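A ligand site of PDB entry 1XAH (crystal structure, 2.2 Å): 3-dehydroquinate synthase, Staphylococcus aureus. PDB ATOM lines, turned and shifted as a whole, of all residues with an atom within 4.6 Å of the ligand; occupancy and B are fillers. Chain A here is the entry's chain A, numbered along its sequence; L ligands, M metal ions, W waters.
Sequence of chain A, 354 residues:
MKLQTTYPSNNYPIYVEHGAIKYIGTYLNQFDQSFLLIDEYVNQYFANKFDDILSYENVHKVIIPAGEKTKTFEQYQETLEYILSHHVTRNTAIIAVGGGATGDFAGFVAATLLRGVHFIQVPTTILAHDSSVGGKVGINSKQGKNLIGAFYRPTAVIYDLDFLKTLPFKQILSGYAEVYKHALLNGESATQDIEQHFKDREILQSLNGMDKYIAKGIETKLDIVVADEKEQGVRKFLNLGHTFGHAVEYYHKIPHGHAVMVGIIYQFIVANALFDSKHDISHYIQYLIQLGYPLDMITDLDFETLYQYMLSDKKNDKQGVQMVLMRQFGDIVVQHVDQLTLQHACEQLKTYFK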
ATOM      1  N   ASP A  39     -16.993 -18.252  -7.469  1.00  0.00           N
ATOM      2  CA  ASP A  39     -17.049 -16.925  -6.849  1.00  0.00           C
ATOM      3  C   ASP A  39     -16.198 -15.895  -7.598  1.00  0.00           C
ATOM      4  O   ASP A  39     -15.091 -16.189  -8.036  1.00  0.00           O
ATOM      5  CB  ASP A  39     -16.575 -17.077  -5.392  1.00  0.00           C
ATOM      6  CG  ASP A  39     -16.686 -15.807  -4.602  1.00  0.00           C
ATOM      7  OD1 ASP A  39     -16.118 -14.784  -5.033  1.00  0.00           O
ATOM      8  OD2 ASP A  39     -17.339 -15.833  -3.529  1.00  0.00           O
ATOM      9  N   TYR A  41     -14.363 -13.275  -6.634  1.00  0.00           N
ATOM     10  CA  TYR A  41     -13.023 -13.153  -6.073  1.00  0.00           C
ATOM     11  C   TYR A  41     -12.296 -14.480  -6.177  1.00  0.00           C
ATOM     12  O   TYR A  41     -11.168 -14.546  -6.681  1.00  0.00           O
ATOM     13  CB  TYR A  41     -13.092 -12.739  -4.593  1.00  0.00           C
ATOM     14  CG  TYR A  41     -13.703 -11.368  -4.325  1.00  0.00           C
ATOM     15  CD1 TYR A  41     -14.098 -11.007  -3.027  1.00  0.00           C
ATOM     16  CD2 TYR A  41     -13.882 -10.430  -5.353  1.00  0.00           C
ATOM     17  CE1 TYR A  41     -14.676  -9.763  -2.759  1.00  0.00           C
ATOM     18  CE2 TYR A  41     -14.461  -9.173  -5.090  1.00  0.00           C
ATOM     19  CZ  TYR A  41     -14.853  -8.847  -3.785  1.00  0.00           C
ATOM     20  OH  TYR A  41     -15.448  -7.627  -3.517  1.00  0.00           O
ATOM     21  N   VAL A  42     -12.922 -15.559  -5.706  1.00  0.00           N
ATOM     22  CA  VAL A  42     -12.308 -16.886  -5.770  1.00  0.00           C
ATOM     23  C   VAL A  42     -11.736 -17.154  -7.155  1.00  0.00           C
ATOM     24  O   VAL A  42     -10.684 -17.802  -7.289  1.00  0.00           O
ATOM     25  CB  VAL A  42     -13.327 -17.989  -5.416  1.00  0.00           C
ATOM     26  CG1 VAL A  42     -12.683 -19.355  -5.582  1.00  0.00           C
ATOM     27  CG2 VAL A  42     -13.791 -17.825  -3.985  1.00  0.00           C
ATOM     28  N   TYR A  45      -8.268 -15.514  -7.454  1.00  0.00           N
ATOM     29  CA  TYR A  45      -7.299 -16.303  -6.715  1.00  0.00           C
ATOM     30  C   TYR A  45      -6.907 -17.628  -7.392  1.00  0.00           C
ATOM     31  O   TYR A  45      -5.721 -17.933  -7.495  1.00  0.00           O
ATOM     32  CB  TYR A  45      -7.865 -16.601  -5.310  1.00  0.00           C
ATOM     33  CG  TYR A  45      -7.599 -15.555  -4.238  1.00  0.00           C
ATOM     34  CD1 TYR A  45      -6.321 -15.400  -3.697  1.00  0.00           C
ATOM     35  CD2 TYR A  45      -8.640 -14.794  -3.696  1.00  0.00           C
ATOM     36  CE1 TYR A  45      -6.090 -14.511  -2.627  1.00  0.00           C
ATOM     37  CE2 TYR A  45      -8.408 -13.905  -2.626  1.00  0.00           C
ATOM     38  CZ  TYR A  45      -7.136 -13.777  -2.097  1.00  0.00           C
ATOM     39  OH  TYR A  45      -6.899 -12.959  -1.014  1.00  0.00           O
ATOM     40  N   PHE A  46      -7.886 -18.402  -7.853  1.00  0.00           N
ATOM     41  CA  PHE A  46      -7.554 -19.700  -8.432  1.00  0.00           C
ATOM     42  C   PHE A  46      -7.971 -20.005  -9.877  1.00  0.00           C
ATOM     43  O   PHE A  46      -8.039 -21.163 -10.264  1.00  0.00           O
ATOM     44  CB  PHE A  46      -8.113 -20.818  -7.541  1.00  0.00           C
ATOM     45  CG  PHE A  46      -8.020 -20.511  -6.070  1.00  0.00           C
ATOM     46  CD1 PHE A  46      -9.096 -19.982  -5.378  1.00  0.00           C
ATOM     47  CD2 PHE A  46      -6.832 -20.750  -5.373  1.00  0.00           C
ATOM     48  CE1 PHE A  46      -9.005 -19.686  -4.010  1.00  0.00           C
ATOM     49  CE2 PHE A  46      -6.721 -20.452  -4.004  1.00  0.00           C
ATOM     50  CZ  PHE A  46      -7.808 -19.916  -3.331  1.00  0.00           C
ATOM     51  N   ALA A  66     -19.639 -12.082  -5.469  1.00  0.00           N
ATOM     52  CA  ALA A  66     -18.788 -12.457  -4.349  1.00  0.00           C
ATOM     53  C   ALA A  66     -19.597 -12.652  -3.080  1.00  0.00           C
ATOM     54  O   ALA A  66     -20.475 -11.862  -2.762  1.00  0.00           O
ATOM     55  CB  ALA A  66     -17.745 -11.381  -4.116  1.00  0.00           C
ATOM     56  N   GLY A  67     -19.273 -13.727  -2.357  1.00  0.00           N
ATOM     57  CA  GLY A  67     -19.960 -14.015  -1.114  1.00  0.00           C
ATOM     58  C   GLY A  67     -21.474 -13.960  -1.168  1.00  0.00           C
ATOM     59  O   GLY A  67     -22.078 -14.432  -2.122  1.00  0.00           O
ATOM     60  N   GLU A  68     -22.066 -13.357  -0.140  1.00  0.00           N
ATOM     61  CA  GLU A  68     -23.525 -13.258  -0.022  1.00  0.00           C
ATOM     62  C   GLU A  68     -24.223 -12.495  -1.158  1.00  0.00           C
ATOM     63  O   GLU A  68     -25.445 -12.578  -1.286  1.00  0.00           O
ATOM     64  CB  GLU A  68     -23.871 -12.602   1.317  1.00  0.00           C
ATOM     65  CG  GLU A  68     -25.277 -12.882   1.829  1.00  0.00           C
ATOM     66  CD  GLU A  68     -25.344 -14.140   2.661  1.00  0.00           C
ATOM     67  OE1 GLU A  68     -26.465 -14.554   3.035  1.00  0.00           O
ATOM     68  OE2 GLU A  68     -24.276 -14.720   2.937  1.00  0.00           O
ATOM     69  N   LYS A  71     -26.427 -14.732  -3.369  1.00  0.00           N
ATOM     70  CA  LYS A  71     -27.604 -15.413  -2.795  1.00  0.00           C
ATOM     71  C   LYS A  71     -28.893 -14.614  -2.830  1.00  0.00           C
ATOM     72  O   LYS A  71     -29.595 -14.496  -1.828  1.00  0.00           O
ATOM     73  CB  LYS A  71     -27.299 -15.871  -1.363  1.00  0.00           C
ATOM     74  CG  LYS A  71     -26.391 -17.091  -1.331  1.00  0.00           C
ATOM     75  CD  LYS A  71     -25.978 -17.504   0.079  1.00  0.00           C
ATOM     76  CE  LYS A  71     -27.133 -18.060   0.881  1.00  0.00           C
ATOM     77  NZ  LYS A  71     -26.655 -18.715   2.135  1.00  0.00           N
ATOM     78  N   GLY A  99     -16.834 -20.430  -1.305  1.00  0.00           N
ATOM     79  CA  GLY A  99     -17.244 -20.570   0.084  1.00  0.00           C
ATOM     80  C   GLY A  99     -18.621 -21.152   0.338  1.00  0.00           C
ATOM     81  O   GLY A  99     -19.145 -21.921  -0.459  1.00  0.00           O
ATOM     82  N   GLY A 100     -19.207 -20.776   1.464  1.00  0.00           N
ATOM     83  CA  GLY A 100     -20.520 -21.273   1.821  1.00  0.00           C
ATOM     84  C   GLY A 100     -21.609 -20.628   0.995  1.00  0.00           C
ATOM     85  O   GLY A 100     -22.599 -21.269   0.656  1.00  0.00           O
ATOM     86  N   ALA A 101     -21.418 -19.338   0.670  1.00  0.00           N
ATOM     87  CA  ALA A 101     -22.382 -18.560  -0.118  1.00  0.00           C
ATOM     88  C   ALA A 101     -22.538 -19.073  -1.537  1.00  0.00           C
ATOM     89  O   ALA A 101     -23.650 -19.090  -2.069  1.00  0.00           O
ATOM     90  CB  ALA A 101     -21.955 -17.102  -0.149  1.00  0.00           C
ATOM     91  N   THR A 102     -21.439 -19.457  -2.177  1.00  0.00           N
ATOM     92  CA  THR A 102     -21.540 -19.964  -3.538  1.00  0.00           C
ATOM     93  C   THR A 102     -22.102 -21.394  -3.487  1.00  0.00           C
ATOM     94  O   THR A 102     -22.947 -21.756  -4.313  1.00  0.00           O
ATOM     95  CB  THR A 102     -20.186 -19.940  -4.237  1.00  0.00           C
ATOM     96  OG1 THR A 102     -19.353 -20.962  -3.687  1.00  0.00           O
ATOM     97  CG2 THR A 102     -19.511 -18.584  -4.056  1.00  0.00           C
ATOM     98  N   ASP A 104     -24.218 -22.748  -1.382  1.00  0.00           N
ATOM     99  CA  ASP A 104     -25.660 -22.689  -1.139  1.00  0.00           C
ATOM    100  C   ASP A 104     -26.424 -22.291  -2.389  1.00  0.00           C
ATOM    101  O   ASP A 104     -27.439 -22.894  -2.724  1.00  0.00           O
ATOM    102  CB  ASP A 104     -25.977 -21.648  -0.081  1.00  0.00           C
ATOM    103  CG  ASP A 104     -25.541 -22.074   1.291  1.00  0.00           C
ATOM    104  OD1 ASP A 104     -25.686 -21.249   2.216  1.00  0.00           O
ATOM    105  OD2 ASP A 104     -25.080 -23.222   1.430  1.00  0.00           O
ATOM    106  N   THR A 124     -13.877 -23.845  -0.370  1.00  0.00           N
ATOM    107  CA  THR A 124     -12.578 -23.187  -0.310  1.00  0.00           C
ATOM    108  C   THR A 124     -12.332 -22.369   0.958  1.00  0.00           C
ATOM    109  O   THR A 124     -11.344 -21.654   1.047  1.00  0.00           O
ATOM    110  CB  THR A 124     -12.361 -22.258  -1.529  1.00  0.00           C
ATOM    111  OG1 THR A 124     -13.327 -21.207  -1.493  1.00  0.00           O
ATOM    112  CG2 THR A 124     -12.549 -23.028  -2.841  1.00  0.00           C
ATOM    113  N   THR A 125     -13.245 -22.437   1.921  1.00  0.00           N
ATOM    114  CA  THR A 125     -13.059 -21.716   3.168  1.00  0.00           C
ATOM    115  C   THR A 125     -13.162 -22.666   4.370  1.00  0.00           C
ATOM    116  O   THR A 125     -13.654 -23.785   4.251  1.00  0.00           O
ATOM    117  CB  THR A 125     -14.105 -20.585   3.378  1.00  0.00           C
ATOM    118  OG1 THR A 125     -15.428 -21.138   3.373  1.00  0.00           O
ATOM    119  CG2 THR A 125     -13.972 -19.503   2.287  1.00  0.00           C
ATOM    120  N   LEU A 127     -15.001 -22.180   7.070  1.00  0.00           N
ATOM    121  CA  LEU A 127     -16.420 -22.204   7.387  1.00  0.00           C
ATOM    122  C   LEU A 127     -17.189 -23.121   6.424  1.00  0.00           C
ATOM    123  O   LEU A 127     -18.317 -23.506   6.702  1.00  0.00           O
ATOM    124  CB  LEU A 127     -16.985 -20.781   7.341  1.00  0.00           C
ATOM    125  CG  LEU A 127     -18.214 -20.454   8.204  1.00  0.00           C
ATOM    126  CD1 LEU A 127     -18.402 -18.951   8.265  1.00  0.00           C
ATOM    127  CD2 LEU A 127     -19.447 -21.129   7.638  1.00  0.00           C
ATOM    128  N   ASP A 130     -18.365 -26.826   7.241  1.00  0.00           N
ATOM    129  CA  ASP A 130     -19.694 -26.989   7.783  1.00  0.00           C
ATOM    130  C   ASP A 130     -20.756 -26.934   6.685  1.00  0.00           C
ATOM    131  O   ASP A 130     -21.548 -27.867   6.551  1.00  0.00           O
ATOM    132  CB  ASP A 130     -19.945 -25.905   8.839  1.00  0.00           C
ATOM    133  CG  ASP A 130     -21.391 -25.850   9.298  1.00  0.00           C
ATOM    134  OD1 ASP A 130     -22.060 -26.909   9.320  1.00  0.00           O
ATOM    135  OD2 ASP A 130     -21.859 -24.760   9.655  1.00  0.00           O
ATOM    136  N   SER A 131     -20.744 -25.858   5.905  1.00  0.00           N
ATOM    137  CA  SER A 131     -21.723 -25.640   4.834  1.00  0.00           C
ATOM    138  C   SER A 131     -21.786 -26.632   3.669  1.00  0.00           C
ATOM    139  O   SER A 131     -22.863 -26.901   3.150  1.00  0.00           O
ATOM    140  CB  SER A 131     -21.570 -24.212   4.273  1.00  0.00           C
ATOM    141  OG  SER A 131     -20.302 -24.021   3.697  1.00  0.00           O
ATOM    142  N   VAL A 133     -21.374 -29.696   3.849  1.00  0.00           N
ATOM    143  CA  VAL A 133     -21.903 -30.966   4.361  1.00  0.00           C
ATOM    144  C   VAL A 133     -23.314 -30.833   4.930  1.00  0.00           C
ATOM    145  O   VAL A 133     -23.610 -29.875   5.648  1.00  0.00           O
ATOM    146  CB  VAL A 133     -20.982 -31.532   5.488  1.00  0.00           C
ATOM    147  CG1 VAL A 133     -21.560 -32.836   6.038  1.00  0.00           C
ATOM    148  CG2 VAL A 133     -19.593 -31.765   4.941  1.00  0.00           C
ATOM    149  N   LYS A 136     -28.026 -28.632   3.013  1.00  0.00           N
ATOM    150  CA  LYS A 136     -28.771 -27.370   3.035  1.00  0.00           C
ATOM    151  C   LYS A 136     -28.233 -26.432   1.969  1.00  0.00           C
ATOM    152  O   LYS A 136     -27.043 -26.120   1.933  1.00  0.00           O
ATOM    153  CB  LYS A 136     -28.669 -26.691   4.405  1.00  0.00           C
ATOM    154  CG  LYS A 136     -29.706 -27.163   5.431  1.00  0.00           C
ATOM    155  CD  LYS A 136     -29.569 -26.377   6.716  1.00  0.00           C
ATOM    156  CE  LYS A 136     -30.782 -26.506   7.601  1.00  0.00           C
ATOM    157  NZ  LYS A 136     -30.705 -25.508   8.704  1.00  0.00           N
ATOM    158  N   LYS A 145     -32.395 -14.140   6.169  1.00  0.00           N
ATOM    159  CA  LYS A 145     -31.402 -15.081   5.702  1.00  0.00           C
ATOM    160  C   LYS A 145     -31.964 -16.443   5.336  1.00  0.00           C
ATOM    161  O   LYS A 145     -32.974 -16.876   5.891  1.00  0.00           O
ATOM    162  CB  LYS A 145     -30.293 -15.266   6.736  1.00  0.00           C
ATOM    163  CG  LYS A 145     -29.203 -14.225   6.628  1.00  0.00           C
ATOM    164  CD  LYS A 145     -27.898 -14.733   7.169  1.00  0.00           C
ATOM    165  CE  LYS A 145     -27.399 -15.938   6.372  1.00  0.00           C
ATOM    166  NZ  LYS A 145     -26.058 -16.353   6.833  1.00  0.00           N
ATOM    167  N   ASN A 146     -31.281 -17.091   4.390  1.00  0.00           N
ATOM    168  CA  ASN A 146     -31.636 -18.419   3.880  1.00  0.00           C
ATOM    169  C   ASN A 146     -33.085 -18.751   4.217  1.00  0.00           C
ATOM    170  O   ASN A 146     -33.359 -19.640   5.017  1.00  0.00           O
ATOM    171  CB  ASN A 146     -30.714 -19.464   4.509  1.00  0.00           C
ATOM    172  CG  ASN A 146     -29.364 -18.899   4.857  1.00  0.00           C
ATOM    173  OD1 ASN A 146     -28.629 -18.433   3.984  1.00  0.00           O
ATOM    174  ND2 ASN A 146     -29.024 -18.922   6.149  1.00  0.00           N
ATOM    175  N   PHE A 163      -6.630 -24.510  -0.471  1.00  0.00           N
ATOM    176  CA  PHE A 163      -7.463 -23.343  -0.796  1.00  0.00           C
ATOM    177  C   PHE A 163      -7.439 -22.356   0.366  1.00  0.00           C
ATOM    178  O   PHE A 163      -7.571 -21.143   0.174  1.00  0.00           O
ATOM    179  CB  PHE A 163      -8.915 -23.775  -1.023  1.00  0.00           C
ATOM    180  CG  PHE A 163      -9.242 -24.204  -2.432  1.00  0.00           C
ATOM    181  CD1 PHE A 163      -8.975 -23.361  -3.513  1.00  0.00           C
ATOM    182  CD2 PHE A 163      -9.889 -25.404  -2.665  1.00  0.00           C
ATOM    183  CE1 PHE A 163      -9.356 -23.722  -4.817  1.00  0.00           C
ATOM    184  CE2 PHE A 163     -10.271 -25.772  -3.951  1.00  0.00           C
ATOM    185  CZ  PHE A 163     -10.004 -24.933  -5.023  1.00  0.00           C
ATOM    186  N   LEU A 164      -7.301 -22.904   1.571  1.00  0.00           N
ATOM    187  CA  LEU A 164      -7.300 -22.135   2.802  1.00  0.00           C
ATOM    188  C   LEU A 164      -6.121 -21.170   2.979  1.00  0.00           C
ATOM    189  O   LEU A 164      -6.249 -20.170   3.676  1.00  0.00           O
ATOM    190  CB  LEU A 164      -7.372 -23.095   4.011  1.00  0.00           C
ATOM    191  CG  LEU A 164      -8.517 -24.129   4.033  1.00  0.00           C
ATOM    192  CD1 LEU A 164      -8.561 -24.778   5.397  1.00  0.00           C
ATOM    193  CD2 LEU A 164      -9.863 -23.495   3.752  1.00  0.00           C
ATOM    194  N   THR A 166      -4.962 -18.810   1.305  1.00  0.00           N
ATOM    195  CA  THR A 166      -5.219 -17.429   0.910  1.00  0.00           C
ATOM    196  C   THR A 166      -6.311 -16.690   1.669  1.00  0.00           C
ATOM    197  O   THR A 166      -6.710 -15.592   1.281  1.00  0.00           O
ATOM    198  CB  THR A 166      -5.538 -17.361  -0.612  1.00  0.00           C
ATOM    199  OG1 THR A 166      -6.579 -18.299  -0.938  1.00  0.00           O
ATOM    200  CG2 THR A 166      -4.301 -17.715  -1.410  1.00  0.00           C
ATOM    201  N   LEU A 167      -6.777 -17.268   2.760  1.00  0.00           N
ATOM    202  CA  LEU A 167      -7.830 -16.649   3.556  1.00  0.00           C
ATOM    203  C   LEU A 167      -7.360 -15.534   4.478  1.00  0.00           C
ATOM    204  O   LEU A 167      -6.499 -15.741   5.333  1.00  0.00           O
ATOM    205  CB  LEU A 167      -8.523 -17.715   4.412  1.00  0.00           C
ATOM    206  CG  LEU A 167      -9.355 -18.783   3.709  1.00  0.00           C
ATOM    207  CD1 LEU A 167      -9.844 -19.786   4.738  1.00  0.00           C
ATOM    208  CD2 LEU A 167     -10.533 -18.130   2.994  1.00  0.00           C
ATOM    209  N   PRO A 168      -7.928 -14.321   4.331  1.00  0.00           N
ATOM    210  CA  PRO A 168      -7.502 -13.244   5.224  1.00  0.00           C
ATOM    211  C   PRO A 168      -7.816 -13.734   6.618  1.00  0.00           C
ATOM    212  O   PRO A 168      -8.489 -14.744   6.781  1.00  0.00           O
ATOM    213  CB  PRO A 168      -8.400 -12.084   4.819  1.00  0.00           C
ATOM    214  CG  PRO A 168      -8.662 -12.338   3.378  1.00  0.00           C
ATOM    215  CD  PRO A 168      -8.888 -13.836   3.331  1.00  0.00           C
ATOM    216  N   GLN A 171     -11.542 -13.999   7.466  1.00  0.00           N
ATOM    217  CA  GLN A 171     -12.258 -15.212   7.062  1.00  0.00           C
ATOM    218  C   GLN A 171     -11.822 -16.387   7.930  1.00  0.00           C
ATOM    219  O   GLN A 171     -12.574 -17.331   8.119  1.00  0.00           O
ATOM    220  CB  GLN A 171     -12.008 -15.513   5.580  1.00  0.00           C
ATOM    221  CG  GLN A 171     -12.485 -14.395   4.655  1.00  0.00           C
ATOM    222  CD  GLN A 171     -13.916 -13.981   4.941  1.00  0.00           C
ATOM    223  OE1 GLN A 171     -14.287 -12.816   4.789  1.00  0.00           O
ATOM    224  NE2 GLN A 171     -14.731 -14.939   5.351  1.00  0.00           N
ATOM    225  N   SER A 174     -13.909 -15.945  11.095  1.00  0.00           N
ATOM    226  CA  SER A 174     -15.280 -16.305  10.748  1.00  0.00           C
ATOM    227  C   SER A 174     -15.471 -17.812  10.633  1.00  0.00           C
ATOM    228  O   SER A 174     -16.426 -18.367  11.158  1.00  0.00           O
ATOM    229  CB  SER A 174     -15.684 -15.642   9.424  1.00  0.00           C
ATOM    230  OG  SER A 174     -17.016 -15.992   9.092  1.00  0.00           O
ATOM    231  N   LYS A 221     -20.514 -33.077  12.702  1.00  0.00           N
ATOM    232  CA  LYS A 221     -21.725 -32.775  11.956  1.00  0.00           C
ATOM    233  C   LYS A 221     -22.225 -33.958  11.135  1.00  0.00           C
ATOM    234  O   LYS A 221     -23.425 -34.135  10.978  1.00  0.00           O
ATOM    235  CB  LYS A 221     -21.494 -31.579  11.036  1.00  0.00           C
ATOM    236  CG  LYS A 221     -22.644 -31.347  10.087  1.00  0.00           C
ATOM    237  CD  LYS A 221     -22.558 -29.999   9.436  1.00  0.00           C
ATOM    238  CE  LYS A 221     -23.714 -29.821   8.507  1.00  0.00           C
ATOM    239  NZ  LYS A 221     -23.775 -28.463   7.944  1.00  0.00           N
ATOM    240  N   ARG A 235     -30.475 -32.274  14.639  1.00  0.00           N
ATOM    241  CA  ARG A 235     -29.752 -31.383  13.742  1.00  0.00           C
ATOM    242  C   ARG A 235     -29.977 -29.938  14.159  1.00  0.00           C
ATOM    243  O   ARG A 235     -29.293 -29.037  13.689  1.00  0.00           O
ATOM    244  CB  ARG A 235     -30.150 -31.571  12.282  1.00  0.00           C
ATOM    245  CG  ARG A 235     -29.370 -30.635  11.373  1.00  0.00           C
ATOM    246  CD  ARG A 235     -29.494 -30.940   9.913  1.00  0.00           C
ATOM    247  NE  ARG A 235     -28.628 -30.054   9.147  1.00  0.00           N
ATOM    248  CZ  ARG A 235     -28.263 -30.248   7.886  1.00  0.00           C
ATOM    249  NH1 ARG A 235     -28.694 -31.311   7.216  1.00  0.00           N
ATOM    250  NH2 ARG A 235     -27.445 -29.387   7.293  1.00  0.00           N
ATOM    251  N   HIS A 256     -20.324 -14.008   9.126  1.00  0.00           N
ATOM    252  CA  HIS A 256     -21.171 -15.046   9.687  1.00  0.00           C
ATOM    253  C   HIS A 256     -20.584 -15.616  10.979  1.00  0.00           C
ATOM    254  O   HIS A 256     -21.234 -15.635  12.011  1.00  0.00           O
ATOM    255  CB  HIS A 256     -21.332 -16.160   8.653  1.00  0.00           C
ATOM    256  CG  HIS A 256     -22.296 -17.232   9.054  1.00  0.00           C
ATOM    257  ND1 HIS A 256     -23.649 -17.000   9.199  1.00  0.00           N
ATOM    258  CD2 HIS A 256     -22.109 -18.543   9.314  1.00  0.00           C
ATOM    259  CE1 HIS A 256     -24.251 -18.127   9.531  1.00  0.00           C
ATOM    260  NE2 HIS A 256     -23.343 -19.078   9.602  1.00  0.00           N
HETATM  261  P1  LIG L   1     -18.446 -16.624   1.503  1.00  0.00           P
HETATM  262  O1  LIG L   1     -18.781 -17.409   0.312  1.00  0.00           O
HETATM  263  O2  LIG L   1     -19.021 -15.260   1.388  1.00  0.00           O
HETATM  264  O3  LIG L   1     -16.832 -16.546   1.660  1.00  0.00           O
HETATM  265  C1  LIG L   1     -16.262 -15.464   2.482  1.00  0.00           C
HETATM  266  C2  LIG L   1     -15.338 -14.657   1.586  1.00  0.00           C
HETATM  267  O4  LIG L   1     -14.160 -15.402   1.229  1.00  0.00           O
HETATM  268  C3  LIG L   1     -15.899 -14.210   0.231  1.00  0.00           C
HETATM  269  O5  LIG L   1     -15.621 -12.805  -0.055  1.00  0.00           O
HETATM  270  C4  LIG L   1     -15.205 -15.089  -0.836  1.00  0.00           C
HETATM  271  O6  LIG L   1     -15.137 -14.444  -2.104  1.00  0.00           O
HETATM  272  C5  LIG L   1     -13.867 -15.282  -0.203  1.00  0.00           C
HETATM  273  N1  LIG L   1     -13.093 -16.520  -0.400  1.00  0.00           N
HETATM  274  C6  LIG L   1     -13.643 -17.775  -0.654  1.00  0.00           C
HETATM  275  N2  LIG L   1     -12.690 -18.697  -0.690  1.00  0.00           N
HETATM  276  C7  LIG L   1     -11.492 -18.022  -0.494  1.00  0.00           C
HETATM  277  C8  LIG L   1     -10.132 -18.457  -0.443  1.00  0.00           C
HETATM  278  N3  LIG L   1      -9.738 -19.723  -0.486  1.00  0.00           N
HETATM  279  N4  LIG L   1      -9.163 -17.459  -0.333  1.00  0.00           N
HETATM  280  C9  LIG L   1      -9.560 -16.158  -0.144  1.00  0.00           C
HETATM  281  N5  LIG L   1     -10.792 -15.647  -0.128  1.00  0.00           N
HETATM  282  C10 LIG L   1     -11.731 -16.675  -0.338  1.00  0.00           C
HETATM  283  O7  LIG L   1     -19.032 -17.332   2.787  1.00  0.00           O
HETATM  284  P2  LIG L   1     -18.451 -18.324   3.910  1.00  0.00           P
HETATM  285  O8  LIG L   1     -17.602 -19.334   3.301  1.00  0.00           O
HETATM  286  O9  LIG L   1     -17.649 -17.554   4.920  1.00  0.00           O
HETATM  287  O10 LIG L   1     -19.717 -19.013   4.631  1.00  0.00           O
HETATM  288  C11 LIG L   1     -20.850 -18.259   5.058  1.00  0.00           C
HETATM  289  C12 LIG L   1     -22.071 -18.558   4.175  1.00  0.00           C
HETATM  290  O11 LIG L   1     -22.441 -19.958   4.319  1.00  0.00           O
HETATM  291  C13 LIG L   1     -23.319 -17.736   4.563  1.00  0.00           C
HETATM  292  O12 LIG L   1     -23.938 -17.307   3.362  1.00  0.00           O
HETATM  293  C14 LIG L   1     -24.151 -18.717   5.409  1.00  0.00           C
HETATM  294  O13 LIG L   1     -25.564 -18.408   5.434  1.00  0.00           O
HETATM  295  C15 LIG L   1     -23.831 -20.072   4.805  1.00  0.00           C
HETATM  296  N6  LIG L   1     -23.792 -21.238   5.711  1.00  0.00           N
HETATM  297  C16 LIG L   1     -24.591 -22.279   5.238  1.00  0.00           C
HETATM  298  C17 LIG L   1     -24.625 -23.489   5.938  1.00  0.00           C
HETATM  299  C18 LIG L   1     -25.311 -24.774   5.352  1.00  0.00           C
HETATM  300  O14 LIG L   1     -25.599 -24.830   4.158  1.00  0.00           O
HETATM  301  N7  LIG L   1     -25.573 -25.812   6.197  1.00  0.00           N
HETATM  302  C19 LIG L   1     -24.021 -23.638   7.248  1.00  0.00           C
HETATM  303  C20 LIG L   1     -23.101 -22.587   7.554  1.00  0.00           C
HETATM  304  C21 LIG L   1     -23.025 -21.350   6.931  1.00  0.00           C
HETATM  305 ZN    ZN M   1     -23.479 -21.622  10.579  1.00  0.00          ZN
HETATM  306  O   HOH W   1     -26.293 -27.066   8.365  1.00  0.00           O
HETATM  307  O   HOH W   2     -25.840 -28.387   5.222  1.00  0.00           O
HETATM  308  O   HOH W   3     -15.010 -17.839   5.216  1.00  0.00           O
HETATM  309  O   HOH W   4     -17.637 -15.416   6.616  1.00  0.00           O
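An oxygen (O13) of the ligand is in hydrogen-bond range of the side-chain amino group (NZ) of Lys 145 (2.5 Å). The side-chain carboxylate (OE2) of Glu 68 sits at hydrogen-bond distance from an oxygen (O12) of the ligand, at 2.6 Å. N3 of the ligand is in hydrogen-bond range of O of Phe 163 (2.7 Å). O of Thr 124 lies within hydrogen-bond range of N3 of the ligand, 2.9 Å away. The side-chain hydroxyl (OG1) of Thr 124 lies within hydrogen-bond range of a nitrogen (N2) of the ligand. The side-chain hydroxyl (OG1) of Thr 166 sits at hydrogen-bond distance from a nitrogen (N4) of the ligand, 2.8 Å away. O8 of the ligand is in hydrogen-bond range of OG1 of Thr 125 (2.8 Å). The backbone NH (N) of Gly 100 lies within hydrogen-bond range of an oxygen (O8) of the ligand (2.8 Å). OD2 of Asp 39 is in hydrogen-bond range of O6 of the ligand (3.0 Å). The backbone NH (N) of Ala 101 lies close to an oxygen (O1) of the ligand, at 3.3 Å. An oxygen (O12) of the ligand is in hydrogen-bond range of the side-chain amino group of Lys 71, 3.3 Å away. O13 of the ligand is in hydrogen-bond range of OD1 of Asn 146 (3.4 Å).
O of Phe 163 is in hydrogen-bond range of OG1 of Thr 166 (3.2 Å). The backbone carbonyl oxygen of Thr 166 is in hydrogen-bond range of the side-chain hydroxyl of Tyr 45 (3.5 Å). The side-chain carboxylate of Asp 39 lies within hydrogen-bond range of the backbone NH of Gly 67 (3.1 Å). OD1 of Asp 39 is in hydrogen-bond range of N of Val 42, 3.4 Å away. The side-chain carboxylate (OD1) of Asp 39 sits at hydrogen-bond distance from the backbone NH (N) of Tyr 41 (2.8 Å). The side-chain amino group of Lys 221 lies within salt-bridge range of the side-chain carboxylate of Asp 130 (2.7 Å). OD1 of Asn 146 is in hydrogen-bond range of NZ of Lys 71 (2.7 Å). O of Gly 99 lies within hydrogen-bond range of OG1 of Thr 102, at 3.4 Å.
An oxygen (O14) of the ligand lies close to the side-chain carboxylate (OD2) of Asp 104, at 3.2 Å. An oxygen (O14) of the ligand sits close to the backbone carbonyl oxygen of Lys 136. Tyr 41 touches the ligand (CB to O6, 3.6 Å). Val 42 touches the ligand. Tyr 45 touches the ligand. Phe 46 touches the ligand (CZ to N3, 3.4 Å). Gly 67 touches the ligand (CA to O2, 2.9 Å). CA of Gly 99 touches O8 of the ligand, 3.5 Å away. CD2 of Leu 127 touches C21 of the ligand, 3.7 Å away. Asp 130 touches the ligand (OD2 to C20, 3.3 Å). Ser 131 touches the ligand. Leu 167 touches the ligand (CD2 to C8, 3.5 Å). Gln 171 touches the ligand. NZ of Lys 221 touches N7 of the ligand, 3.6 Å away. His 256 touches the ligand (NE2 to C21, 3.5 Å). The nearest printed residue that does not touch the ligand is Thr 102 (4.2 Å).
Water W3 bridges an oxygen (O9) of the ligand (2.7 Å) and the side-chain amide nitrogen of Gln 171 (2.9 Å). Water W4 lies within hydrogen-bond range of OG of Ser 174, O9 of the ligand and NE2 of Gln 171.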
